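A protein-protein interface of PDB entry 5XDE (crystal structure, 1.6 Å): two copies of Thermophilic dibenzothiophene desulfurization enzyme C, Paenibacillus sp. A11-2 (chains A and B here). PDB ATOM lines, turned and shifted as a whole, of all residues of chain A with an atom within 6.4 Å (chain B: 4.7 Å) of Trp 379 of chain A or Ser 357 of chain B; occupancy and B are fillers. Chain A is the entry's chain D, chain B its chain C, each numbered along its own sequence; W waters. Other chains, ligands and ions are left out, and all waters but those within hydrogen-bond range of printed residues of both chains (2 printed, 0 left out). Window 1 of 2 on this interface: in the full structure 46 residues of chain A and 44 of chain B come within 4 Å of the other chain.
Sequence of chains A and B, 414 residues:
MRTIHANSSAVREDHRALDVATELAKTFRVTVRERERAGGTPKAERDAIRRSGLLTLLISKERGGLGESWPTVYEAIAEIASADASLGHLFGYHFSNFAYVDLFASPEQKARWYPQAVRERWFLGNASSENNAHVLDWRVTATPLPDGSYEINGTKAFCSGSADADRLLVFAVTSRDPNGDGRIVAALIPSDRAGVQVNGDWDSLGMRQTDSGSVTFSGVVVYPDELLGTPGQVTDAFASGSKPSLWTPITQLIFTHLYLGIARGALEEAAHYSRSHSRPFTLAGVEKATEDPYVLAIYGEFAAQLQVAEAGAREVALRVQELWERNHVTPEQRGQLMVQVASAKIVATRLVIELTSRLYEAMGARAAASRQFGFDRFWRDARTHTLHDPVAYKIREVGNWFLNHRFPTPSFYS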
ATOM      1  N   LEU A 205      11.567   5.265 -14.767  1.00  0.00           N
ATOM      2  CA  LEU A 205      13.019   5.428 -14.723  1.00  0.00           C
ATOM      3  C   LEU A 205      13.558   5.192 -13.316  1.00  0.00           C
ATOM      4  O   LEU A 205      14.505   4.420 -13.113  1.00  0.00           O
ATOM      5  CB  LEU A 205      13.377   6.829 -15.206  1.00  0.00           C
ATOM      6  CG  LEU A 205      14.831   7.300 -15.170  1.00  0.00           C
ATOM      7  CD1 LEU A 205      15.706   6.456 -16.099  1.00  0.00           C
ATOM      8  CD2 LEU A 205      14.893   8.784 -15.542  1.00  0.00           C
ATOM      9  N   ILE A 262      17.700  11.277  -0.373  1.00  0.00           N
ATOM     10  CA  ILE A 262      18.437  10.778  -1.535  1.00  0.00           C
ATOM     11  C   ILE A 262      19.803  11.442  -1.629  1.00  0.00           C
ATOM     12  O   ILE A 262      20.807  10.779  -1.923  1.00  0.00           O
ATOM     13  CB  ILE A 262      17.627  10.976  -2.831  1.00  0.00           C
ATOM     14  CG1 ILE A 262      16.365  10.103  -2.793  1.00  0.00           C
ATOM     15  CG2 ILE A 262      18.516  10.649  -4.083  1.00  0.00           C
ATOM     16  CD1 ILE A 262      15.371  10.401  -3.915  1.00  0.00           C
ATOM     17  N   ALA A 266      23.278   9.341  -1.537  1.00  0.00           N
ATOM     18  CA  ALA A 266      24.181   9.357  -2.685  1.00  0.00           C
ATOM     19  C   ALA A 266      25.576   9.825  -2.285  1.00  0.00           C
ATOM     20  O   ALA A 266      26.581   9.231  -2.696  1.00  0.00           O
ATOM     21  CB  ALA A 266      23.598  10.250  -3.786  1.00  0.00           C
ATOM     22  N   VAL A 352      19.917  17.909  -5.103  1.00  0.00           N
ATOM     23  CA  VAL A 352      19.940  16.468  -5.347  1.00  0.00           C
ATOM     24  C   VAL A 352      20.173  16.183  -6.828  1.00  0.00           C
ATOM     25  O   VAL A 352      20.907  15.253  -7.184  1.00  0.00           O
ATOM     26  CB  VAL A 352      18.653  15.802  -4.827  1.00  0.00           C
ATOM     27  CG1 VAL A 352      17.451  16.152  -5.678  1.00  0.00           C
ATOM     28  CG2 VAL A 352      18.851  14.268  -4.760  1.00  0.00           C
ATOM     29  N   ILE A 353      19.578  16.989  -7.708  1.00  0.00           N
ATOM     30  CA  ILE A 353      19.748  16.775  -9.145  1.00  0.00           C
ATOM     31  C   ILE A 353      21.200  16.989  -9.558  1.00  0.00           C
ATOM     32  O   ILE A 353      21.741  16.235 -10.382  1.00  0.00           O
ATOM     33  CB  ILE A 353      18.788  17.683  -9.938  1.00  0.00           C
ATOM     34  CG1 ILE A 353      17.340  17.215  -9.735  1.00  0.00           C
ATOM     35  CG2 ILE A 353      19.140  17.640 -11.415  1.00  0.00           C
ATOM     36  CD1 ILE A 353      17.141  15.745 -10.063  1.00  0.00           C
ATOM     37  N   GLU A 354      21.857  18.005  -8.993  1.00  0.00           N
ATOM     38  CA  GLU A 354      23.253  18.265  -9.326  1.00  0.00           C
ATOM     39  C   GLU A 354      24.177  17.195  -8.748  1.00  0.00           C
ATOM     40  O   GLU A 354      25.027  16.642  -9.461  1.00  0.00           O
ATOM     41  CB  GLU A 354      23.658  19.661  -8.841  1.00  0.00           C
ATOM     42  CG  GLU A 354      25.121  20.020  -9.101  1.00  0.00           C
ATOM     43  CD  GLU A 354      25.397  20.509 -10.523  1.00  0.00           C
ATOM     44  OE1 GLU A 354      26.539  20.970 -10.776  1.00  0.00           O
ATOM     45  OE2 GLU A 354      24.484  20.438 -11.383  1.00  0.00           O
ATOM     46  N   THR A 356      23.696  14.061  -7.606  1.00  0.00           N
ATOM     47  CA  THR A 356      23.577  12.669  -8.043  1.00  0.00           C
ATOM     48  C   THR A 356      24.212  12.452  -9.409  1.00  0.00           C
ATOM     49  O   THR A 356      24.573  11.321  -9.738  1.00  0.00           O
ATOM     50  CB  THR A 356      22.120  12.195  -8.067  1.00  0.00           C
ATOM     51  OG1 THR A 356      21.317  13.067  -8.870  1.00  0.00           O
ATOM     52  CG2 THR A 356      21.554  12.166  -6.660  1.00  0.00           C
ATOM     53  N   SER A 357      24.399  13.511 -10.186  1.00  0.00           N
ATOM     54  CA  SER A 357      25.097  13.438 -11.462  1.00  0.00           C
ATOM     55  C   SER A 357      26.588  13.747 -11.311  1.00  0.00           C
ATOM     56  O   SER A 357      27.441  12.981 -11.779  1.00  0.00           O
ATOM     57  CB  SER A 357      24.436  14.398 -12.455  1.00  0.00           C
ATOM     58  OG  SER A 357      25.172  14.476 -13.659  1.00  0.00           O
ATOM     59  N   TYR A 360      29.844  11.464  -9.852  1.00  0.00           N
ATOM     60  CA  TYR A 360      30.669  10.548 -10.635  1.00  0.00           C
ATOM     61  C   TYR A 360      32.068  11.106 -10.844  1.00  0.00           C
ATOM     62  O   TYR A 360      33.041  10.342 -10.913  1.00  0.00           O
ATOM     63  CB  TYR A 360      30.023  10.249 -11.991  1.00  0.00           C
ATOM     64  CG  TYR A 360      28.971   9.163 -11.948  1.00  0.00           C
ATOM     65  CD1 TYR A 360      29.321   7.824 -12.064  1.00  0.00           C
ATOM     66  CD2 TYR A 360      27.625   9.475 -11.815  1.00  0.00           C
ATOM     67  CE1 TYR A 360      28.351   6.823 -12.036  1.00  0.00           C
ATOM     68  CE2 TYR A 360      26.659   8.492 -11.792  1.00  0.00           C
ATOM     69  CZ  TYR A 360      27.027   7.166 -11.905  1.00  0.00           C
ATOM     70  OH  TYR A 360      26.081   6.166 -11.883  1.00  0.00           O
ATOM     71  N   PHE A 375      25.095   3.058  -9.032  1.00  0.00           N
ATOM     72  CA  PHE A 375      25.012   4.371  -8.405  1.00  0.00           C
ATOM     73  C   PHE A 375      24.002   5.264  -9.102  1.00  0.00           C
ATOM     74  O   PHE A 375      23.467   6.189  -8.472  1.00  0.00           O
ATOM     75  CB  PHE A 375      26.391   5.039  -8.400  1.00  0.00           C
ATOM     76  CG  PHE A 375      26.431   6.362  -7.659  1.00  0.00           C
ATOM     77  CD1 PHE A 375      26.576   6.401  -6.280  1.00  0.00           C
ATOM     78  CD2 PHE A 375      26.335   7.563  -8.358  1.00  0.00           C
ATOM     79  CE1 PHE A 375      26.614   7.618  -5.604  1.00  0.00           C
ATOM     80  CE2 PHE A 375      26.371   8.782  -7.689  1.00  0.00           C
ATOM     81  CZ  PHE A 375      26.515   8.809  -6.313  1.00  0.00           C
ATOM     82  N   ASP A 376      23.719   5.000 -10.377  1.00  0.00           N
ATOM     83  CA  ASP A 376      22.773   5.818 -11.123  1.00  0.00           C
ATOM     84  C   ASP A 376      21.375   5.762 -10.541  1.00  0.00           C
ATOM     85  O   ASP A 376      20.537   6.591 -10.920  1.00  0.00           O
ATOM     86  CB  ASP A 376      22.731   5.375 -12.582  1.00  0.00           C
ATOM     87  CG  ASP A 376      22.274   3.945 -12.738  1.00  0.00           C
ATOM     88  OD1 ASP A 376      22.969   3.043 -12.207  1.00  0.00           O
ATOM     89  OD2 ASP A 376      21.223   3.724 -13.380  1.00  0.00           O
ATOM     90  N   ARG A 377      21.102   4.809  -9.640  1.00  0.00           N
ATOM     91  CA  ARG A 377      19.793   4.736  -9.004  1.00  0.00           C
ATOM     92  C   ARG A 377      19.448   6.054  -8.319  1.00  0.00           C
ATOM     93  O   ARG A 377      18.296   6.499  -8.346  1.00  0.00           O
ATOM     94  CB  ARG A 377      19.777   3.585  -7.997  1.00  0.00           C
ATOM     95  CG  ARG A 377      18.506   3.472  -7.190  1.00  0.00           C
ATOM     96  CD  ARG A 377      18.538   2.214  -6.331  1.00  0.00           C
ATOM     97  NE  ARG A 377      19.730   2.176  -5.490  1.00  0.00           N
ATOM     98  CZ  ARG A 377      19.801   2.733  -4.282  1.00  0.00           C
ATOM     99  NH1 ARG A 377      18.737   3.362  -3.771  1.00  0.00           N
ATOM    100  NH2 ARG A 377      20.926   2.661  -3.583  1.00  0.00           N
ATOM    101  N   PHE A 378      20.441   6.711  -7.730  1.00  0.00           N
ATOM    102  CA  PHE A 378      20.147   7.953  -7.022  1.00  0.00           C
ATOM    103  C   PHE A 378      19.671   9.029  -7.989  1.00  0.00           C
ATOM    104  O   PHE A 378      18.637   9.670  -7.754  1.00  0.00           O
ATOM    105  CB  PHE A 378      21.368   8.420  -6.238  1.00  0.00           C
ATOM    106  CG  PHE A 378      21.778   7.474  -5.147  1.00  0.00           C
ATOM    107  CD1 PHE A 378      21.107   7.445  -3.935  1.00  0.00           C
ATOM    108  CD2 PHE A 378      22.855   6.611  -5.341  1.00  0.00           C
ATOM    109  CE1 PHE A 378      21.496   6.571  -2.926  1.00  0.00           C
ATOM    110  CE2 PHE A 378      23.252   5.740  -4.350  1.00  0.00           C
ATOM    111  CZ  PHE A 378      22.577   5.712  -3.139  1.00  0.00           C
ATOM    112  N   TRP A 379      20.388   9.222  -9.103  1.00  0.00           N
ATOM    113  CA  TRP A 379      19.932  10.202 -10.088  1.00  0.00           C
ATOM    114  C   TRP A 379      18.579   9.799 -10.674  1.00  0.00           C
ATOM    115  O   TRP A 379      17.679  10.633 -10.815  1.00  0.00           O
ATOM    116  CB  TRP A 379      20.982  10.382 -11.197  1.00  0.00           C
ATOM    117  CG  TRP A 379      20.488  11.282 -12.320  1.00  0.00           C
ATOM    118  CD1 TRP A 379      20.539  12.651 -12.355  1.00  0.00           C
ATOM    119  CD2 TRP A 379      19.849  10.872 -13.542  1.00  0.00           C
ATOM    120  NE1 TRP A 379      19.978  13.119 -13.532  1.00  0.00           N
ATOM    121  CE2 TRP A 379      19.552  12.045 -14.276  1.00  0.00           C
ATOM    122  CE3 TRP A 379      19.505   9.629 -14.091  1.00  0.00           C
ATOM    123  CZ2 TRP A 379      18.935  12.007 -15.525  1.00  0.00           C
ATOM    124  CZ3 TRP A 379      18.884   9.594 -15.325  1.00  0.00           C
ATOM    125  CH2 TRP A 379      18.606  10.775 -16.031  1.00  0.00           C
ATOM    126  N   ARG A 380      18.397   8.512 -10.985  1.00  0.00           N
ATOM    127  CA  ARG A 380      17.127   8.084 -11.554  1.00  0.00           C
ATOM    128  C   ARG A 380      15.975   8.375 -10.597  1.00  0.00           C
ATOM    129  O   ARG A 380      14.938   8.917 -11.004  1.00  0.00           O
ATOM    130  CB  ARG A 380      17.173   6.596 -11.913  1.00  0.00           C
ATOM    131  CG  ARG A 380      18.022   6.277 -13.150  1.00  0.00           C
ATOM    132  CD  ARG A 380      17.867   4.806 -13.594  1.00  0.00           C
ATOM    133  NE  ARG A 380      18.541   3.826 -12.736  1.00  0.00           N
ATOM    134  CZ  ARG A 380      17.934   3.056 -11.826  1.00  0.00           C
ATOM    135  NH1 ARG A 380      16.626   3.137 -11.611  1.00  0.00           N
ATOM    136  NH2 ARG A 380      18.644   2.197 -11.109  1.00  0.00           N
ATOM    137  N   ASP A 381      16.158   8.067  -9.315  1.00  0.00           N
ATOM    138  CA  ASP A 381      15.103   8.307  -8.334  1.00  0.00           C
ATOM    139  C   ASP A 381      14.808   9.798  -8.201  1.00  0.00           C
ATOM    140  O   ASP A 381      13.646  10.227  -8.239  1.00  0.00           O
ATOM    141  CB  ASP A 381      15.514   7.723  -6.975  1.00  0.00           C
ATOM    142  CG  ASP A 381      15.512   6.200  -6.953  1.00  0.00           C
ATOM    143  OD1 ASP A 381      14.871   5.566  -7.824  1.00  0.00           O
ATOM    144  OD2 ASP A 381      16.168   5.639  -6.045  1.00  0.00           O
ATOM    145  N   ALA A 382      15.858  10.605  -8.062  1.00  0.00           N
ATOM    146  CA  ALA A 382      15.662  12.034  -7.848  1.00  0.00           C
ATOM    147  C   ALA A 382      15.136  12.710  -9.107  1.00  0.00           C
ATOM    148  O   ALA A 382      14.222  13.544  -9.037  1.00  0.00           O
ATOM    149  CB  ALA A 382      16.977  12.669  -7.395  1.00  0.00           C
ATOM    150  N   ARG A 383      15.675  12.337 -10.271  1.00  0.00           N
ATOM    151  CA  ARG A 383      15.229  12.945 -11.518  1.00  0.00           C
ATOM    152  C   ARG A 383      13.756  12.668 -11.751  1.00  0.00           C
ATOM    153  O   ARG A 383      13.025  13.526 -12.268  1.00  0.00           O
ATOM    154  CB  ARG A 383      16.059  12.417 -12.689  1.00  0.00           C
ATOM    155  CG  ARG A 383      15.677  13.025 -14.034  1.00  0.00           C
ATOM    156  CD  ARG A 383      15.984  14.521 -14.138  1.00  0.00           C
ATOM    157  NE  ARG A 383      15.018  15.340 -13.396  1.00  0.00           N
ATOM    158  CZ  ARG A 383      15.071  16.662 -13.314  1.00  0.00           C
ATOM    159  NH1 ARG A 383      16.021  17.336 -13.962  1.00  0.00           N
ATOM    160  NH2 ARG A 383      14.171  17.315 -12.592  1.00  0.00           N
ATOM    161  N   THR A 384      13.296  11.473 -11.364  1.00  0.00           N
ATOM    162  CA  THR A 384      11.896  11.123 -11.556  1.00  0.00           C
ATOM    163  C   THR A 384      11.008  11.914 -10.609  1.00  0.00           C
ATOM    164  O   THR A 384      10.051  12.578 -11.033  1.00  0.00           O
ATOM    165  CB  THR A 384      11.692   9.624 -11.343  1.00  0.00           C
ATOM    166  OG1 THR A 384      12.419   8.898 -12.345  1.00  0.00           O
ATOM    167  CG2 THR A 384      10.214   9.264 -11.431  1.00  0.00           C
ATOM    168  N   ILE B 353      26.407  17.192 -19.789  1.00  0.00           N
ATOM    169  CA  ILE B 353      25.990  16.652 -18.493  1.00  0.00           C
ATOM    170  C   ILE B 353      24.813  17.444 -17.923  1.00  0.00           C
ATOM    171  O   ILE B 353      23.891  16.864 -17.340  1.00  0.00           O
ATOM    172  CB  ILE B 353      27.174  16.610 -17.516  1.00  0.00           C
ATOM    173  CG1 ILE B 353      28.207  15.589 -18.007  1.00  0.00           C
ATOM    174  CG2 ILE B 353      26.700  16.281 -16.101  1.00  0.00           C
ATOM    175  CD1 ILE B 353      27.691  14.150 -18.080  1.00  0.00           C
ATOM    176  N   GLU B 354      24.826  18.775 -18.058  1.00  0.00           N
ATOM    177  CA  GLU B 354      23.704  19.565 -17.542  1.00  0.00           C
ATOM    178  C   GLU B 354      22.448  19.336 -18.366  1.00  0.00           C
ATOM    179  O   GLU B 354      21.360  19.118 -17.825  1.00  0.00           O
ATOM    180  CB  GLU B 354      24.043  21.056 -17.545  1.00  0.00           C
ATOM    181  CG  GLU B 354      25.198  21.471 -16.675  1.00  0.00           C
ATOM    182  CD  GLU B 354      25.417  22.974 -16.705  1.00  0.00           C
ATOM    183  OE1 GLU B 354      26.339  23.468 -16.013  1.00  0.00           O
ATOM    184  OE2 GLU B 354      24.658  23.663 -17.427  1.00  0.00           O
ATOM    185  N   LEU B 355      22.581  19.408 -19.682  1.00  0.00           N
ATOM    186  CA  LEU B 355      21.419  19.393 -20.553  1.00  0.00           C
ATOM    187  C   LEU B 355      20.692  18.048 -20.510  1.00  0.00           C
ATOM    188  O   LEU B 355      19.456  18.008 -20.474  1.00  0.00           O
ATOM    189  CB  LEU B 355      21.901  19.761 -21.959  1.00  0.00           C
ATOM    190  CG  LEU B 355      21.247  19.517 -23.310  1.00  0.00           C
ATOM    191  CD1 LEU B 355      22.116  20.261 -24.326  1.00  0.00           C
ATOM    192  CD2 LEU B 355      21.164  18.036 -23.640  1.00  0.00           C
ATOM    193  N   THR B 356      21.438  16.935 -20.509  1.00  0.00           N
ATOM    194  CA  THR B 356      20.793  15.626 -20.562  1.00  0.00           C
ATOM    195  C   THR B 356      20.003  15.329 -19.293  1.00  0.00           C
ATOM    196  O   THR B 356      19.086  14.499 -19.326  1.00  0.00           O
ATOM    197  CB  THR B 356      21.824  14.508 -20.816  1.00  0.00           C
ATOM    198  OG1 THR B 356      22.845  14.521 -19.806  1.00  0.00           O
ATOM    199  CG2 THR B 356      22.497  14.714 -22.186  1.00  0.00           C
ATOM    200  N   SER B 357      20.313  16.005 -18.190  1.00  0.00           N
ATOM    201  CA  SER B 357      19.543  15.881 -16.958  1.00  0.00           C
ATOM    202  C   SER B 357      18.456  16.948 -16.856  1.00  0.00           C
ATOM    203  O   SER B 357      17.300  16.641 -16.552  1.00  0.00           O
ATOM    204  CB  SER B 357      20.485  15.964 -15.752  1.00  0.00           C
ATOM    205  OG  SER B 357      19.778  15.984 -14.526  1.00  0.00           O
ATOM    206  N   ARG B 358      18.800  18.210 -17.116  1.00  0.00           N
ATOM    207  CA  ARG B 358      17.839  19.283 -16.876  1.00  0.00           C
ATOM    208  C   ARG B 358      16.706  19.309 -17.901  1.00  0.00           C
ATOM    209  O   ARG B 358      15.654  19.875 -17.607  1.00  0.00           O
ATOM    210  CB  ARG B 358      18.556  20.636 -16.854  1.00  0.00           C
ATOM    211  CG  ARG B 358      19.674  20.786 -15.787  1.00  0.00           C
ATOM    212  CD  ARG B 358      19.182  21.219 -14.399  1.00  0.00           C
ATOM    213  NE  ARG B 358      18.014  22.098 -14.446  1.00  0.00           N
ATOM    214  CZ  ARG B 358      18.047  23.371 -14.832  1.00  0.00           C
ATOM    215  NH1 ARG B 358      19.195  23.919 -15.215  1.00  0.00           N
ATOM    216  NH2 ARG B 358      16.930  24.094 -14.846  1.00  0.00           N
ATOM    217  N   LEU B 359      16.885  18.725 -19.094  1.00  0.00           N
ATOM    218  CA  LEU B 359      15.815  18.795 -20.085  1.00  0.00           C
ATOM    219  C   LEU B 359      14.537  18.100 -19.621  1.00  0.00           C
ATOM    220  O   LEU B 359      13.464  18.406 -20.150  1.00  0.00           O
ATOM    221  CB  LEU B 359      16.278  18.208 -21.426  1.00  0.00           C
ATOM    222  CG  LEU B 359      16.967  19.230 -22.336  1.00  0.00           C
ATOM    223  CD1 LEU B 359      17.692  18.539 -23.492  1.00  0.00           C
ATOM    224  CD2 LEU B 359      15.958  20.229 -22.866  1.00  0.00           C
ATOM    225  N   TYR B 360      14.609  17.183 -18.651  1.00  0.00           N
ATOM    226  CA  TYR B 360      13.365  16.619 -18.126  1.00  0.00           C
ATOM    227  C   TYR B 360      12.435  17.715 -17.622  1.00  0.00           C
ATOM    228  O   TYR B 360      11.205  17.597 -17.730  1.00  0.00           O
ATOM    229  CB  TYR B 360      13.663  15.621 -17.005  1.00  0.00           C
ATOM    230  CG  TYR B 360      14.061  14.236 -17.489  1.00  0.00           C
ATOM    231  CD1 TYR B 360      13.095  13.265 -17.757  1.00  0.00           C
ATOM    232  CD2 TYR B 360      15.396  13.900 -17.693  1.00  0.00           C
ATOM    233  CE1 TYR B 360      13.442  12.000 -18.186  1.00  0.00           C
ATOM    234  CE2 TYR B 360      15.752  12.635 -18.131  1.00  0.00           C
ATOM    235  CZ  TYR B 360      14.774  11.691 -18.384  1.00  0.00           C
ATOM    236  OH  TYR B 360      15.137  10.426 -18.809  1.00  0.00           O
ATOM    237  N   ASP B 376      16.696   8.823 -20.842  1.00  0.00           N
ATOM    238  CA  ASP B 376      17.862   8.761 -19.976  1.00  0.00           C
ATOM    239  C   ASP B 376      19.089   8.180 -20.671  1.00  0.00           C
ATOM    240  O   ASP B 376      20.190   8.282 -20.124  1.00  0.00           O
ATOM    241  CB  ASP B 376      17.559   7.925 -18.731  1.00  0.00           C
ATOM    242  CG  ASP B 376      17.169   6.502 -19.069  1.00  0.00           C
ATOM    243  OD1 ASP B 376      16.178   6.307 -19.831  1.00  0.00           O
ATOM    244  OD2 ASP B 376      17.860   5.583 -18.559  1.00  0.00           O
ATOM    245  N   TRP B 379      21.803  10.928 -20.985  1.00  0.00           N
ATOM    246  CA  TRP B 379      22.587  11.173 -19.774  1.00  0.00           C
ATOM    247  C   TRP B 379      23.493   9.985 -19.455  1.00  0.00           C
ATOM    248  O   TRP B 379      24.673  10.161 -19.117  1.00  0.00           O
ATOM    249  CB  TRP B 379      21.663  11.478 -18.584  1.00  0.00           C
ATOM    250  CG  TRP B 379      22.387  11.609 -17.289  1.00  0.00           C
ATOM    251  CD1 TRP B 379      22.977  12.738 -16.790  1.00  0.00           C
ATOM    252  CD2 TRP B 379      22.625  10.571 -16.322  1.00  0.00           C
ATOM    253  NE1 TRP B 379      23.578  12.465 -15.576  1.00  0.00           N
ATOM    254  CE2 TRP B 379      23.375  11.145 -15.267  1.00  0.00           C
ATOM    255  CE3 TRP B 379      22.272   9.217 -16.243  1.00  0.00           C
ATOM    256  CZ2 TRP B 379      23.763  10.414 -14.133  1.00  0.00           C
ATOM    257  CZ3 TRP B 379      22.668   8.484 -15.125  1.00  0.00           C
ATOM    258  CH2 TRP B 379      23.410   9.082 -14.087  1.00  0.00           C
HETATM  259  O   HOH W   1      23.930  16.763 -14.639  1.00  0.00           O
HETATM  260  O   HOH W   2      21.970  17.027 -13.033  1.00  0.00           O
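Of the printed residues of chain B, Trp 379 of chain A touches Ser 357 (3.0 Å) and Trp 379 (3.5 Å).
Ser 357 of chain B touches just these residues of chain A: Ile 353 (3.6 Å), Trp 379 (3.0 Å) and Arg 383 (3.0 Å).
Of the printed residues of chain B, Arg 383 of chain A touches Ser 357, Arg 358 and Tyr 360.
Of the printed residues of chain B, Leu 205 of chain A touches Tyr 360 (3.7 Å) and Asp 376 (3.3 Å).
Arg 380 of chain A touches none of the printed residues of chain B.
The nearest residue of chain A that does not touch Ser 357 of chain B is Ser 357 of chain A (5.3 Å).
The nearest printed residue of chain A that does not touch Asp 376 of chain B is Trp 379 of chain A (4.02 Å).
Ile 353 of chain A touches Ser 357 of chain B, and with the chains exchanged Ser 357 of chain A touches Ile 353 of chain B.
Ser 357 of chain A touches Trp 379 of chain B, and with the chains exchanged Trp 379 of chain A touches Ser 357 of chain B.
Trp 379 of chain A touches its own counterpart, Trp 379 of chain B.
Of the 10 pairs that touch across the chains among the printed residues, 5 have their exchanged pair printed and touching as well.
O of Leu 205 of chain A is in hydrogen-bond range of NH1 of Arg 380 of chain A.
OH of Tyr 360 of chain B is in hydrogen-bond range of N of Asp 376 of chain B (3.0 Å).
Water W1 bridges O of Ile 353 of chain B (2.7 Å) and OG of Ser 357 of chain A (2.8 Å).
Water W2 bridges O of Ile 353 of chain A and OG of Ser 357 of chain B.
Of the 10 printed residues of chain B, 6 touch a printed residue of chain A.
Among the printed residues, 10 pairs touch across the chains.
Among the printed residues, pairs that only touch across the chains: Leu 205 of chain A with Tyr 360 of chain B, Leu 205 of chain A with Asp 376 of chain B, Ile 353 of chain A with Ser 357 of chain B, Ser 357 of chain A with Ile 353 of chain B, Trp 379 of chain A with Trp 379 of chain B, Arg 383 of chain A with Arg 358 of chain B and Arg 383 of chain A with Tyr 360 of chain B.
The side-chain hydroxyl of Ser 357 of chain B lies within hydrogen-bond range of the indole nitrogen of Trp 379 of chain A (3.0 Å).
The indole nitrogen (NE1) of Trp 379 of chain B sits at hydrogen-bond distance from the side-chain hydroxyl (OG) of Ser 357 of chain A (3.2 Å).
NH1 of Arg 383 of chain A lies within hydrogen-bond range of O of Ser 357 of chain B, at 3.0 Å.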
